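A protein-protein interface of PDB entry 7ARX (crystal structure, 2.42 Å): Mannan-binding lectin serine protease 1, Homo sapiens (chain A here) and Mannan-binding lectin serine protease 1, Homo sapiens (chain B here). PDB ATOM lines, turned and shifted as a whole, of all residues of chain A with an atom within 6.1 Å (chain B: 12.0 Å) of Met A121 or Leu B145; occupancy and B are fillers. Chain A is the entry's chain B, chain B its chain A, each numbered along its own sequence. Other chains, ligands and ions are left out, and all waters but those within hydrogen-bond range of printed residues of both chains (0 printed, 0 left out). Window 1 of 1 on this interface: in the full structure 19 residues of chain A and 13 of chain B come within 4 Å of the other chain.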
ATOM      1  N   PRO A  13      25.769 -23.624  32.189  1.00  0.00           N
ATOM      2  CA  PRO A  13      24.411 -23.113  31.967  1.00  0.00           C
ATOM      3  C   PRO A  13      23.508 -24.049  31.179  1.00  0.00           C
ATOM      4  O   PRO A  13      22.329 -23.728  30.991  1.00  0.00           O
ATOM      5  CB  PRO A  13      24.666 -21.816  31.188  1.00  0.00           C
ATOM      6  CG  PRO A  13      25.908 -22.101  30.419  1.00  0.00           C
ATOM      7  CD  PRO A  13      26.750 -23.007  31.279  1.00  0.00           C
ATOM      8  N   TRP A  14      24.021 -25.187  30.716  1.00  0.00           N
ATOM      9  CA  TRP A  14      23.239 -26.142  29.945  1.00  0.00           C
ATOM     10  C   TRP A  14      22.682 -27.281  30.785  1.00  0.00           C
ATOM     11  O   TRP A  14      21.791 -27.996  30.314  1.00  0.00           O
ATOM     12  CB  TRP A  14      24.090 -26.722  28.810  1.00  0.00           C
ATOM     13  CG  TRP A  14      25.534 -26.847  29.176  1.00  0.00           C
ATOM     14  CD1 TRP A  14      26.115 -27.849  29.896  1.00  0.00           C
ATOM     15  CD2 TRP A  14      26.581 -25.928  28.848  1.00  0.00           C
ATOM     16  NE1 TRP A  14      27.462 -27.613  30.033  1.00  0.00           N
ATOM     17  CE2 TRP A  14      27.773 -26.440  29.398  1.00  0.00           C
ATOM     18  CE3 TRP A  14      26.629 -24.723  28.141  1.00  0.00           C
ATOM     19  CZ2 TRP A  14      28.997 -25.789  29.262  1.00  0.00           C
ATOM     20  CZ3 TRP A  14      27.845 -24.079  28.008  1.00  0.00           C
ATOM     21  CH2 TRP A  14      29.012 -24.612  28.566  1.00  0.00           C
ATOM     22  N   ILE A  15      23.181 -27.469  32.008  1.00  0.00           N
ATOM     23  CA  ILE A  15      22.732 -28.583  32.830  1.00  0.00           C
ATOM     24  C   ILE A  15      21.279 -28.365  33.235  1.00  0.00           C
ATOM     25  O   ILE A  15      20.841 -27.232  33.479  1.00  0.00           O
ATOM     26  CB  ILE A  15      23.649 -28.755  34.056  1.00  0.00           C
ATOM     27  CG1 ILE A  15      23.336 -30.062  34.789  1.00  0.00           C
ATOM     28  CG2 ILE A  15      23.532 -27.566  35.004  1.00  0.00           C
ATOM     29  N   LEU A  31      20.472 -29.079  28.210  1.00  0.00           N
ATOM     30  CA  LEU A  31      19.650 -28.298  27.297  1.00  0.00           C
ATOM     31  C   LEU A  31      20.200 -28.399  25.881  1.00  0.00           C
ATOM     32  O   LEU A  31      21.385 -28.148  25.643  1.00  0.00           O
ATOM     33  CB  LEU A  31      19.592 -26.840  27.744  1.00  0.00           C
ATOM     34  CG  LEU A  31      18.840 -25.900  26.802  1.00  0.00           C
ATOM     35  CD1 LEU A  31      17.395 -26.342  26.625  1.00  0.00           C
ATOM     36  CD2 LEU A  31      18.907 -24.473  27.316  1.00  0.00           C
ATOM     37  N   GLY A  33      19.238 -27.128  21.881  1.00  0.00           N
ATOM     38  CA  GLY A  33      18.374 -26.249  21.115  1.00  0.00           C
ATOM     39  C   GLY A  33      17.695 -25.236  22.013  1.00  0.00           C
ATOM     40  O   GLY A  33      18.313 -24.636  22.900  1.00  0.00           O
ATOM     41  N   LEU A 116      16.650 -17.695  27.123  1.00  0.00           N
ATOM     42  CA  LEU A 116      18.085 -17.904  26.972  1.00  0.00           C
ATOM     43  C   LEU A 116      18.846 -16.698  27.504  1.00  0.00           C
ATOM     44  O   LEU A 116      18.737 -15.596  26.958  1.00  0.00           O
ATOM     45  CB  LEU A 116      18.432 -18.156  25.508  1.00  0.00           C
ATOM     46  CG  LEU A 116      18.354 -19.593  24.986  1.00  0.00           C
ATOM     47  CD1 LEU A 116      16.954 -20.179  25.124  1.00  0.00           C
ATOM     48  CD2 LEU A 116      18.807 -19.634  23.539  1.00  0.00           C
ATOM     49  N   ASN A 117      19.616 -16.907  28.567  1.00  0.00           N
ATOM     50  CA  ASN A 117      20.424 -15.850  29.160  1.00  0.00           C
ATOM     51  C   ASN A 117      21.779 -16.443  29.527  1.00  0.00           C
ATOM     52  O   ASN A 117      22.090 -17.590  29.190  1.00  0.00           O
ATOM     53  CB  ASN A 117      19.709 -15.231  30.368  1.00  0.00           C
ATOM     54  CG  ASN A 117      19.438 -16.241  31.459  1.00  0.00           C
ATOM     55  OD1 ASN A 117      20.251 -16.424  32.366  1.00  0.00           O
ATOM     56  ND2 ASN A 117      18.294 -16.909  31.378  1.00  0.00           N
ATOM     57  N   ALA A 118      22.591 -15.653  30.234  1.00  0.00           N
ATOM     58  CA  ALA A 118      23.933 -16.089  30.605  1.00  0.00           C
ATOM     59  C   ALA A 118      23.931 -17.289  31.542  1.00  0.00           C
ATOM     60  O   ALA A 118      24.994 -17.883  31.759  1.00  0.00           O
ATOM     61  CB  ALA A 118      24.697 -14.931  31.249  1.00  0.00           C
ATOM     62  N   PHE A 119      22.777 -17.662  32.098  1.00  0.00           N
ATOM     63  CA  PHE A 119      22.674 -18.821  32.971  1.00  0.00           C
ATOM     64  C   PHE A 119      21.865 -19.961  32.371  1.00  0.00           C
ATOM     65  O   PHE A 119      21.825 -21.045  32.963  1.00  0.00           O
ATOM     66  CB  PHE A 119      22.061 -18.419  34.319  1.00  0.00           C
ATOM     67  CG  PHE A 119      22.881 -17.419  35.082  1.00  0.00           C
ATOM     68  CD1 PHE A 119      23.937 -17.833  35.877  1.00  0.00           C
ATOM     69  CD2 PHE A 119      22.599 -16.066  35.001  1.00  0.00           C
ATOM     70  CE1 PHE A 119      24.696 -16.916  36.578  1.00  0.00           C
ATOM     71  CE2 PHE A 119      23.355 -15.144  35.700  1.00  0.00           C
ATOM     72  CZ  PHE A 119      24.405 -15.571  36.490  1.00  0.00           C
ATOM     73  N   VAL A 120      21.219 -19.750  31.226  1.00  0.00           N
ATOM     74  CA  VAL A 120      20.458 -20.791  30.542  1.00  0.00           C
ATOM     75  C   VAL A 120      20.779 -20.695  29.056  1.00  0.00           C
ATOM     76  O   VAL A 120      20.370 -19.735  28.392  1.00  0.00           O
ATOM     77  CB  VAL A 120      18.944 -20.671  30.772  1.00  0.00           C
ATOM     78  CG1 VAL A 120      18.201 -21.703  29.934  1.00  0.00           C
ATOM     79  CG2 VAL A 120      18.609 -20.842  32.245  1.00  0.00           C
ATOM     80  N   MET A 121      21.507 -21.680  28.535  1.00  0.00           N
ATOM     81  CA  MET A 121      21.821 -21.749  27.115  1.00  0.00           C
ATOM     82  C   MET A 121      22.175 -23.188  26.781  1.00  0.00           C
ATOM     83  O   MET A 121      22.692 -23.910  27.641  1.00  0.00           O
ATOM     84  CB  MET A 121      22.976 -20.804  26.752  1.00  0.00           C
ATOM     85  CG  MET A 121      24.296 -21.157  27.395  1.00  0.00           C
ATOM     86  SD  MET A 121      25.575 -19.956  26.995  1.00  0.00           S
ATOM     87  CE  MET A 121      24.890 -18.477  27.737  1.00  0.00           C
ATOM     88  N   PRO A 122      21.907 -23.638  25.557  1.00  0.00           N
ATOM     89  CA  PRO A 122      22.088 -25.058  25.235  1.00  0.00           C
ATOM     90  C   PRO A 122      23.558 -25.432  25.109  1.00  0.00           C
ATOM     91  O   PRO A 122      24.455 -24.590  25.060  1.00  0.00           O
ATOM     92  CB  PRO A 122      21.360 -25.206  23.898  1.00  0.00           C
ATOM     93  CG  PRO A 122      21.486 -23.860  23.272  1.00  0.00           C
ATOM     94  CD  PRO A 122      21.385 -22.878  24.408  1.00  0.00           C
ATOM     95  N   ILE A 123      23.789 -26.743  25.063  1.00  0.00           N
ATOM     96  CA  ILE A 123      25.111 -27.313  24.834  1.00  0.00           C
ATOM     97  C   ILE A 123      25.162 -27.826  23.403  1.00  0.00           C
ATOM     98  O   ILE A 123      24.160 -28.300  22.853  1.00  0.00           O
ATOM     99  CB  ILE A 123      25.426 -28.432  25.853  1.00  0.00           C
ATOM    100  CG1 ILE A 123      26.882 -28.886  25.736  1.00  0.00           C
ATOM    101  CG2 ILE A 123      24.477 -29.608  25.683  1.00  0.00           C
ATOM    102  CD1 ILE A 123      27.877 -27.840  26.166  1.00  0.00           C
ATOM    103  N   CYS A 124      26.332 -27.712  22.780  1.00  0.00           N
ATOM    104  CA  CYS A 124      26.458 -28.109  21.386  1.00  0.00           C
ATOM    105  C   CYS A 124      26.483 -29.628  21.250  1.00  0.00           C
ATOM    106  O   CYS A 124      26.699 -30.369  22.214  1.00  0.00           O
ATOM    107  CB  CYS A 124      27.720 -27.517  20.761  1.00  0.00           C
ATOM    108  SG  CYS A 124      27.793 -25.717  20.755  1.00  0.00           S
ATOM    109  N   ARG A 209      36.750 -23.990  17.799  1.00  0.00           N
ATOM    110  CA  ARG A 209      35.570 -23.135  17.843  1.00  0.00           C
ATOM    111  C   ARG A 209      35.377 -22.464  19.195  1.00  0.00           C
ATOM    112  O   ARG A 209      34.610 -21.499  19.287  1.00  0.00           O
ATOM    113  CB  ARG A 209      34.318 -23.943  17.491  1.00  0.00           C
ATOM    114  CG  ARG A 209      34.318 -24.516  16.081  1.00  0.00           C
ATOM    115  CD  ARG A 209      34.583 -23.434  15.044  1.00  0.00           C
ATOM    116  NE  ARG A 209      34.566 -23.959  13.680  1.00  0.00           N
ATOM    117  CZ  ARG A 209      33.539 -23.835  12.843  1.00  0.00           C
ATOM    118  NH1 ARG A 209      32.442 -23.198  13.225  1.00  0.00           N
ATOM    119  NH2 ARG A 209      33.614 -24.346  11.622  1.00  0.00           N
ATOM    120  N   GLY A 210      36.048 -22.945  20.239  1.00  0.00           N
ATOM    121  CA  GLY A 210      35.866 -22.376  21.559  1.00  0.00           C
ATOM    122  C   GLY A 210      34.520 -22.655  22.182  1.00  0.00           C
ATOM    123  O   GLY A 210      34.085 -21.903  23.057  1.00  0.00           O
ATOM    124  N   GLN A 211      33.844 -23.717  21.758  1.00  0.00           N
ATOM    125  CA  GLN A 211      32.533 -24.075  22.277  1.00  0.00           C
ATOM    126  C   GLN A 211      32.603 -25.420  22.981  1.00  0.00           C
ATOM    127  O   GLN A 211      33.310 -26.331  22.536  1.00  0.00           O
ATOM    128  CB  GLN A 211      31.488 -24.150  21.160  1.00  0.00           C
ATOM    129  CG  GLN A 211      31.354 -22.897  20.323  1.00  0.00           C
ATOM    130  CD  GLN A 211      30.343 -23.069  19.210  1.00  0.00           C
ATOM    131  OE1 GLN A 211      30.707 -23.290  18.055  1.00  0.00           O
ATOM    132  NE2 GLN A 211      29.065 -22.977  19.555  1.00  0.00           N
ATOM    133  N   TRP A 212      31.863 -25.541  24.077  1.00  0.00           N
ATOM    134  CA  TRP A 212      31.692 -26.827  24.730  1.00  0.00           C
ATOM    135  C   TRP A 212      30.596 -27.614  24.024  1.00  0.00           C
ATOM    136  O   TRP A 212      29.606 -27.045  23.557  1.00  0.00           O
ATOM    137  CB  TRP A 212      31.343 -26.636  26.207  1.00  0.00           C
ATOM    138  CG  TRP A 212      32.379 -25.868  26.968  1.00  0.00           C
ATOM    139  CD1 TRP A 212      32.512 -24.512  27.031  1.00  0.00           C
ATOM    140  CD2 TRP A 212      33.427 -26.412  27.780  1.00  0.00           C
ATOM    141  NE1 TRP A 212      33.580 -24.176  27.829  1.00  0.00           N
ATOM    142  CE2 TRP A 212      34.157 -25.325  28.301  1.00  0.00           C
ATOM    143  CE3 TRP A 212      33.818 -27.711  28.115  1.00  0.00           C
ATOM    144  CZ2 TRP A 212      35.257 -25.499  29.138  1.00  0.00           C
ATOM    145  CZ3 TRP A 212      34.910 -27.880  28.947  1.00  0.00           C
ATOM    146  CH2 TRP A 212      35.616 -26.781  29.449  1.00  0.00           C
ATOM    147  N   HIS B  82      13.367 -13.599  17.929  1.00  0.00           N
ATOM    148  CA  HIS B  82      14.729 -13.573  18.461  1.00  0.00           C
ATOM    149  C   HIS B  82      15.670 -12.773  17.563  1.00  0.00           C
ATOM    150  O   HIS B  82      16.871 -13.048  17.505  1.00  0.00           O
ATOM    151  CB  HIS B  82      15.270 -14.991  18.671  1.00  0.00           C
ATOM    152  CG  HIS B  82      14.320 -15.901  19.385  1.00  0.00           C
ATOM    153  ND1 HIS B  82      13.522 -15.477  20.426  1.00  0.00           N
ATOM    154  CD2 HIS B  82      14.035 -17.212  19.203  1.00  0.00           C
ATOM    155  CE1 HIS B  82      12.791 -16.489  20.857  1.00  0.00           C
ATOM    156  NE2 HIS B  82      13.083 -17.553  20.132  1.00  0.00           N
ATOM    157  N   GLN B 105      19.381 -11.705  17.727  1.00  0.00           N
ATOM    158  CA  GLN B 105      19.759 -11.141  19.018  1.00  0.00           C
ATOM    159  C   GLN B 105      20.970 -11.872  19.583  1.00  0.00           C
ATOM    160  O   GLN B 105      20.830 -12.882  20.279  1.00  0.00           O
ATOM    161  CB  GLN B 105      18.575 -11.191  19.987  1.00  0.00           C
ATOM    162  CG  GLN B 105      17.468 -10.207  19.631  1.00  0.00           C
ATOM    163  CD  GLN B 105      16.258 -10.311  20.541  1.00  0.00           C
ATOM    164  OE1 GLN B 105      16.122 -11.261  21.312  1.00  0.00           O
ATOM    165  NE2 GLN B 105      15.369  -9.328  20.453  1.00  0.00           N
ATOM    166  N   GLU B 106      22.161 -11.365  19.275  1.00  0.00           N
ATOM    167  CA  GLU B 106      23.393 -11.987  19.720  1.00  0.00           C
ATOM    168  C   GLU B 106      23.620 -11.709  21.205  1.00  0.00           C
ATOM    169  O   GLU B 106      23.068 -10.755  21.759  1.00  0.00           O
ATOM    170  CB  GLU B 106      24.563 -11.469  18.885  1.00  0.00           C
ATOM    171  CG  GLU B 106      24.463 -11.803  17.405  1.00  0.00           C
ATOM    172  N   PRO B 107      24.427 -12.543  21.885  1.00  0.00           N
ATOM    173  CA  PRO B 107      25.120 -13.729  21.369  1.00  0.00           C
ATOM    174  C   PRO B 107      24.325 -15.018  21.535  1.00  0.00           C
ATOM    175  O   PRO B 107      24.731 -16.054  21.012  1.00  0.00           O
ATOM    176  CB  PRO B 107      26.385 -13.771  22.221  1.00  0.00           C
ATOM    177  CG  PRO B 107      25.922 -13.265  23.547  1.00  0.00           C
ATOM    178  CD  PRO B 107      24.844 -12.236  23.265  1.00  0.00           C
ATOM    179  N   TYR B 108      23.204 -14.951  22.256  1.00  0.00           N
ATOM    180  CA  TYR B 108      22.452 -16.159  22.574  1.00  0.00           C
ATOM    181  C   TYR B 108      21.741 -16.745  21.361  1.00  0.00           C
ATOM    182  O   TYR B 108      21.321 -17.906  21.408  1.00  0.00           O
ATOM    183  CB  TYR B 108      21.443 -15.868  23.685  1.00  0.00           C
ATOM    184  CG  TYR B 108      22.062 -15.220  24.903  1.00  0.00           C
ATOM    185  CD1 TYR B 108      22.909 -15.936  25.739  1.00  0.00           C
ATOM    186  CD2 TYR B 108      21.800 -13.892  25.216  1.00  0.00           C
ATOM    187  CE1 TYR B 108      23.480 -15.348  26.850  1.00  0.00           C
ATOM    188  CE2 TYR B 108      22.365 -13.296  26.328  1.00  0.00           C
ATOM    189  CZ  TYR B 108      23.203 -14.028  27.142  1.00  0.00           C
ATOM    190  OH  TYR B 108      23.768 -13.438  28.249  1.00  0.00           O
ATOM    191  N   TYR B 109      21.599 -15.979  20.281  1.00  0.00           N
ATOM    192  CA  TYR B 109      20.970 -16.460  19.060  1.00  0.00           C
ATOM    193  C   TYR B 109      21.842 -16.113  17.863  1.00  0.00           C
ATOM    194  O   TYR B 109      22.471 -15.050  17.826  1.00  0.00           O
ATOM    195  CB  TYR B 109      19.569 -15.868  18.880  1.00  0.00           C
ATOM    196  CG  TYR B 109      18.560 -16.375  19.884  1.00  0.00           C
ATOM    197  CD1 TYR B 109      17.905 -17.585  19.689  1.00  0.00           C
ATOM    198  CD2 TYR B 109      18.262 -15.647  21.027  1.00  0.00           C
ATOM    199  CE1 TYR B 109      16.981 -18.053  20.604  1.00  0.00           C
ATOM    200  CE2 TYR B 109      17.339 -16.107  21.947  1.00  0.00           C
ATOM    201  CZ  TYR B 109      16.702 -17.311  21.731  1.00  0.00           C
ATOM    202  OH  TYR B 109      15.783 -17.771  22.646  1.00  0.00           O
ATOM    203  N   LYS B 110      21.877 -17.020  16.889  1.00  0.00           N
ATOM    204  CA  LYS B 110      22.664 -16.847  15.677  1.00  0.00           C
ATOM    205  C   LYS B 110      21.806 -17.175  14.464  1.00  0.00           C
ATOM    206  O   LYS B 110      20.920 -18.031  14.523  1.00  0.00           O
ATOM    207  CB  LYS B 110      23.916 -17.733  15.687  1.00  0.00           C
ATOM    208  N   LEU B 140      18.698 -19.278  15.351  1.00  0.00           N
ATOM    209  CA  LEU B 140      18.912 -20.494  16.115  1.00  0.00           C
ATOM    210  C   LEU B 140      19.714 -20.199  17.379  1.00  0.00           C
ATOM    211  O   LEU B 140      20.556 -19.297  17.391  1.00  0.00           O
ATOM    212  CB  LEU B 140      19.651 -21.546  15.280  1.00  0.00           C
ATOM    213  N   PRO B 141      19.468 -20.936  18.461  1.00  0.00           N
ATOM    214  CA  PRO B 141      20.225 -20.702  19.697  1.00  0.00           C
ATOM    215  C   PRO B 141      21.700 -21.028  19.522  1.00  0.00           C
ATOM    216  O   PRO B 141      22.067 -21.991  18.846  1.00  0.00           O
ATOM    217  CB  PRO B 141      19.565 -21.652  20.705  1.00  0.00           C
ATOM    218  CG  PRO B 141      18.214 -21.938  20.141  1.00  0.00           C
ATOM    219  CD  PRO B 141      18.389 -21.921  18.653  1.00  0.00           C
ATOM    220  N   VAL B 142      22.545 -20.211  20.142  1.00  0.00           N
ATOM    221  CA  VAL B 142      23.978 -20.470  20.202  1.00  0.00           C
ATOM    222  C   VAL B 142      24.257 -21.343  21.415  1.00  0.00           C
ATOM    223  O   VAL B 142      23.643 -21.173  22.474  1.00  0.00           O
ATOM    224  CB  VAL B 142      24.775 -19.154  20.263  1.00  0.00           C
ATOM    225  N   CYS B 143      25.189 -22.278  21.266  1.00  0.00           N
ATOM    226  CA  CYS B 143      25.456 -23.276  22.288  1.00  0.00           C
ATOM    227  C   CYS B 143      26.915 -23.219  22.732  1.00  0.00           C
ATOM    228  O   CYS B 143      27.789 -22.733  22.011  1.00  0.00           O
ATOM    229  CB  CYS B 143      25.121 -24.685  21.775  1.00  0.00           C
ATOM    230  SG  CYS B 143      25.929 -25.123  20.211  1.00  0.00           S
ATOM    231  N   GLY B 144      27.157 -23.720  23.945  1.00  0.00           N
ATOM    232  CA  GLY B 144      28.495 -24.003  24.432  1.00  0.00           C
ATOM    233  C   GLY B 144      29.390 -22.808  24.656  1.00  0.00           C
ATOM    234  O   GLY B 144      30.609 -22.979  24.767  1.00  0.00           O
ATOM    235  N   LEU B 145      28.832 -21.601  24.722  1.00  0.00           N
ATOM    236  CA  LEU B 145      29.608 -20.388  24.959  1.00  0.00           C
ATOM    237  C   LEU B 145      29.207 -19.783  26.297  1.00  0.00           C
ATOM    238  O   LEU B 145      28.393 -18.848  26.346  1.00  0.00           O
ATOM    239  CB  LEU B 145      29.406 -19.378  23.827  1.00  0.00           C
ATOM    240  CG  LEU B 145      30.149 -19.691  22.532  1.00  0.00           C
ATOM    241  N   PRO B 146      29.759 -20.259  27.407  1.00  0.00           N
ATOM    242  CA  PRO B 146      29.394 -19.696  28.707  1.00  0.00           C
ATOM    243  C   PRO B 146      30.061 -18.350  28.943  1.00  0.00           C
ATOM    244  O   PRO B 146      31.178 -18.087  28.492  1.00  0.00           O
ATOM    245  CB  PRO B 146      29.894 -20.750  29.702  1.00  0.00           C
ATOM    246  CG  PRO B 146      30.944 -21.546  28.953  1.00  0.00           C
ATOM    247  CD  PRO B 146      30.910 -21.171  27.498  1.00  0.00           C
ATOM    248  N   LYS B 147      29.347 -17.489  29.663  1.00  0.00           N
ATOM    249  CA  LYS B 147      29.799 -16.130  29.923  1.00  0.00           C
ATOM    250  C   LYS B 147      30.597 -16.014  31.214  1.00  0.00           C
ATOM    251  O   LYS B 147      30.847 -14.896  31.676  1.00  0.00           O
ATOM    252  CB  LYS B 147      28.604 -15.174  29.966  1.00  0.00           C
ATOM    253  CG  LYS B 147      27.583 -15.403  28.863  1.00  0.00           C
ATOM    254  CD  LYS B 147      28.229 -15.368  27.489  1.00  0.00           C
ATOM    255  CE  LYS B 147      27.237 -15.757  26.407  1.00  0.00           C
ATOM    256  NZ  LYS B 147      27.906 -15.917  25.087  1.00  0.00           N
ATOM    257  N   PHE B 148      30.998 -17.136  31.805  1.00  0.00           N
ATOM    258  CA  PHE B 148      31.738 -17.131  33.059  1.00  0.00           C
ATOM    259  C   PHE B 148      32.889 -18.119  32.964  1.00  0.00           C
ATOM    260  O   PHE B 148      32.688 -19.279  32.590  1.00  0.00           O
ATOM    261  CB  PHE B 148      30.826 -17.482  34.240  1.00  0.00           C
ATOM    262  CG  PHE B 148      29.650 -16.561  34.388  1.00  0.00           C
ATOM    263  CD1 PHE B 148      29.779 -15.355  35.055  1.00  0.00           C
ATOM    264  CD2 PHE B 148      28.416 -16.899  33.859  1.00  0.00           C
ATOM    265  CE1 PHE B 148      28.699 -14.503  35.191  1.00  0.00           C
ATOM    266  CE2 PHE B 148      27.333 -16.052  33.992  1.00  0.00           C
ATOM    267  CZ  PHE B 148      27.475 -14.853  34.659  1.00  0.00           C
ATOM    268  N   SER B 149      34.089 -17.656  33.305  1.00  0.00           N
ATOM    269  CA  SER B 149      35.276 -18.491  33.254  1.00  0.00           C
ATOM    270  C   SER B 149      35.412 -19.309  34.536  1.00  0.00           C
ATOM    271  O   SER B 149      34.693 -19.107  35.519  1.00  0.00           O
ATOM    272  CB  SER B 149      36.524 -17.634  33.034  1.00  0.00           C
ATOM    273  N   ARG B 150      36.354 -20.247  34.515  1.00  0.00           N
ATOM    274  CA  ARG B 150      36.638 -21.100  35.659  1.00  0.00           C
ATOM    275  C   ARG B 150      37.865 -20.585  36.398  1.00  0.00           C
ATOM    276  O   ARG B 150      38.819 -20.103  35.782  1.00  0.00           O
ATOM    277  CB  ARG B 150      36.866 -22.548  35.220  1.00  0.00           C
ATOM    278  CG  ARG B 150      35.677 -23.178  34.517  1.00  0.00           C
ATOM    279  CD  ARG B 150      35.928 -24.645  34.212  1.00  0.00           C
ATOM    280  NE  ARG B 150      34.771 -25.272  33.582  1.00  0.00           N
ATOM    281  CZ  ARG B 150      33.741 -25.782  34.251  1.00  0.00           C
ATOM    282  NH1 ARG B 150      33.725 -25.739  35.577  1.00  0.00           N
ATOM    283  NH2 ARG B 150      32.728 -26.332  33.596  1.00  0.00           N
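The backbone carbonyl oxygen (O) of Pro A122 is in hydrogen-bond range of the backbone NH (N) of Gly B144 (3.0 Å). The side-chain hydroxyl of Tyr B108 is in hydrogen-bond range of the backbone NH of Ala A118 (3.2 Å). The backbone carbonyl oxygen of Gly B144 is in hydrogen-bond range of the backbone NH of Trp A212. The backbone carbonyl oxygen of Cys B143 is in hydrogen-bond range of the side-chain amide nitrogen of Gln A211, 2.8 Å away. The side-chain sulfur (SG) of Cys B143 is disulfide-bonded to the side-chain sulfur (SG) of Cys A124, 2.0 Å away. SD of Met A121 sits close to O of Leu B145, 3.1 Å away.
Among the printed residues, pairs that only touch across the chains: Trp A14 with Gly B144 (3.6 Å), Trp A14 with Pro B146 (3.6 Å), Gly A33 with Pro B141 (3.8 Å), Leu A116 with Tyr B108 (3.7 Å), Leu A116 with Tyr B109 (3.6 Å), Leu A116 with Pro B141 (3.6 Å), Asn A117 with Tyr B108 (3.4 Å), Ala A118 with Lys B147 (3.8 Å), Ala A118 with Phe B148 (3.7 Å), Phe A119 with Phe B148 (3.6 Å), Met A121 with Tyr B108 (3.5 Å), Met A121 with Lys B147 (3.8 Å), Pro A122 with Pro B141 (3.9 Å), Pro A122 with Val B142 (3.4 Å), Pro A122 with Cys B143 (3.2 Å), Ile A123 with Cys B143 (3.5 Å), Cys A124 with Gly B144 (3.8 Å), Gln A211 with Gly B144 (3.3 Å) and Trp A212 with Pro B146 (3.7 Å).
No residue of chain B comes within 4 Å of Pro A13. Trp A14 touches two residues of chain B. No residue of chain B comes within 4 Å of Leu A31. Of chain B, only Pro B141 comes within 4 Å of Gly A33. Gly A210 touches none of the printed residues of chain B. Gln A211 touches two residues of chain B. Gln B105 touches none of the printed residues of chain A. Printed residues of chain A within 4 Å of Tyr B109: Leu A116. Of the printed residues of chain A, Leu B145 touches Met A121 (3.1 Å). Of the printed residues of chain A, Lys B147 touches Ala A118 (3.8 Å) and Met A121 (3.8 Å). The nearest residue of chain B that does not touch Met A121 is Pro B146 (4.2 Å). The nearest residue of chain A that does not touch Leu B145 is Gln A211 (4.1 Å).
NE2 of Gln A211 lies within hydrogen-bond range of SG of Cys A124, at 3.3 Å. The backbone carbonyl oxygen (O) of Trp A14 is in hydrogen-bond range of the backbone NH (N) of Leu A31. The backbone carbonyl oxygen (O) of Tyr B108 sits at hydrogen-bond distance from the backbone NH (N) of Val B142, at 2.9 Å. The backbone carbonyl oxygen (O) of Leu B145 sits at hydrogen-bond distance from the side-chain amino group (NZ) of Lys B147, at 3.2 Å. The backbone carbonyl oxygen (O) of Leu A31 sits at hydrogen-bond distance from the backbone NH (N) of Ile A123 (2.8 Å). O of Trp A212 lies close to N of Cys A124 (3.4 Å).
Of the 18 printed residues of chain B, 10 touch a printed residue of chain A. Hydrophobic or aromatic side chains of chain A within 4 Å of the printed part of chain B: Trp A14, Leu A116, Ala A118, Phe A119, Met A121, Pro A122 and Trp A212. Among the printed residues, 25 pairs touch across the chains.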
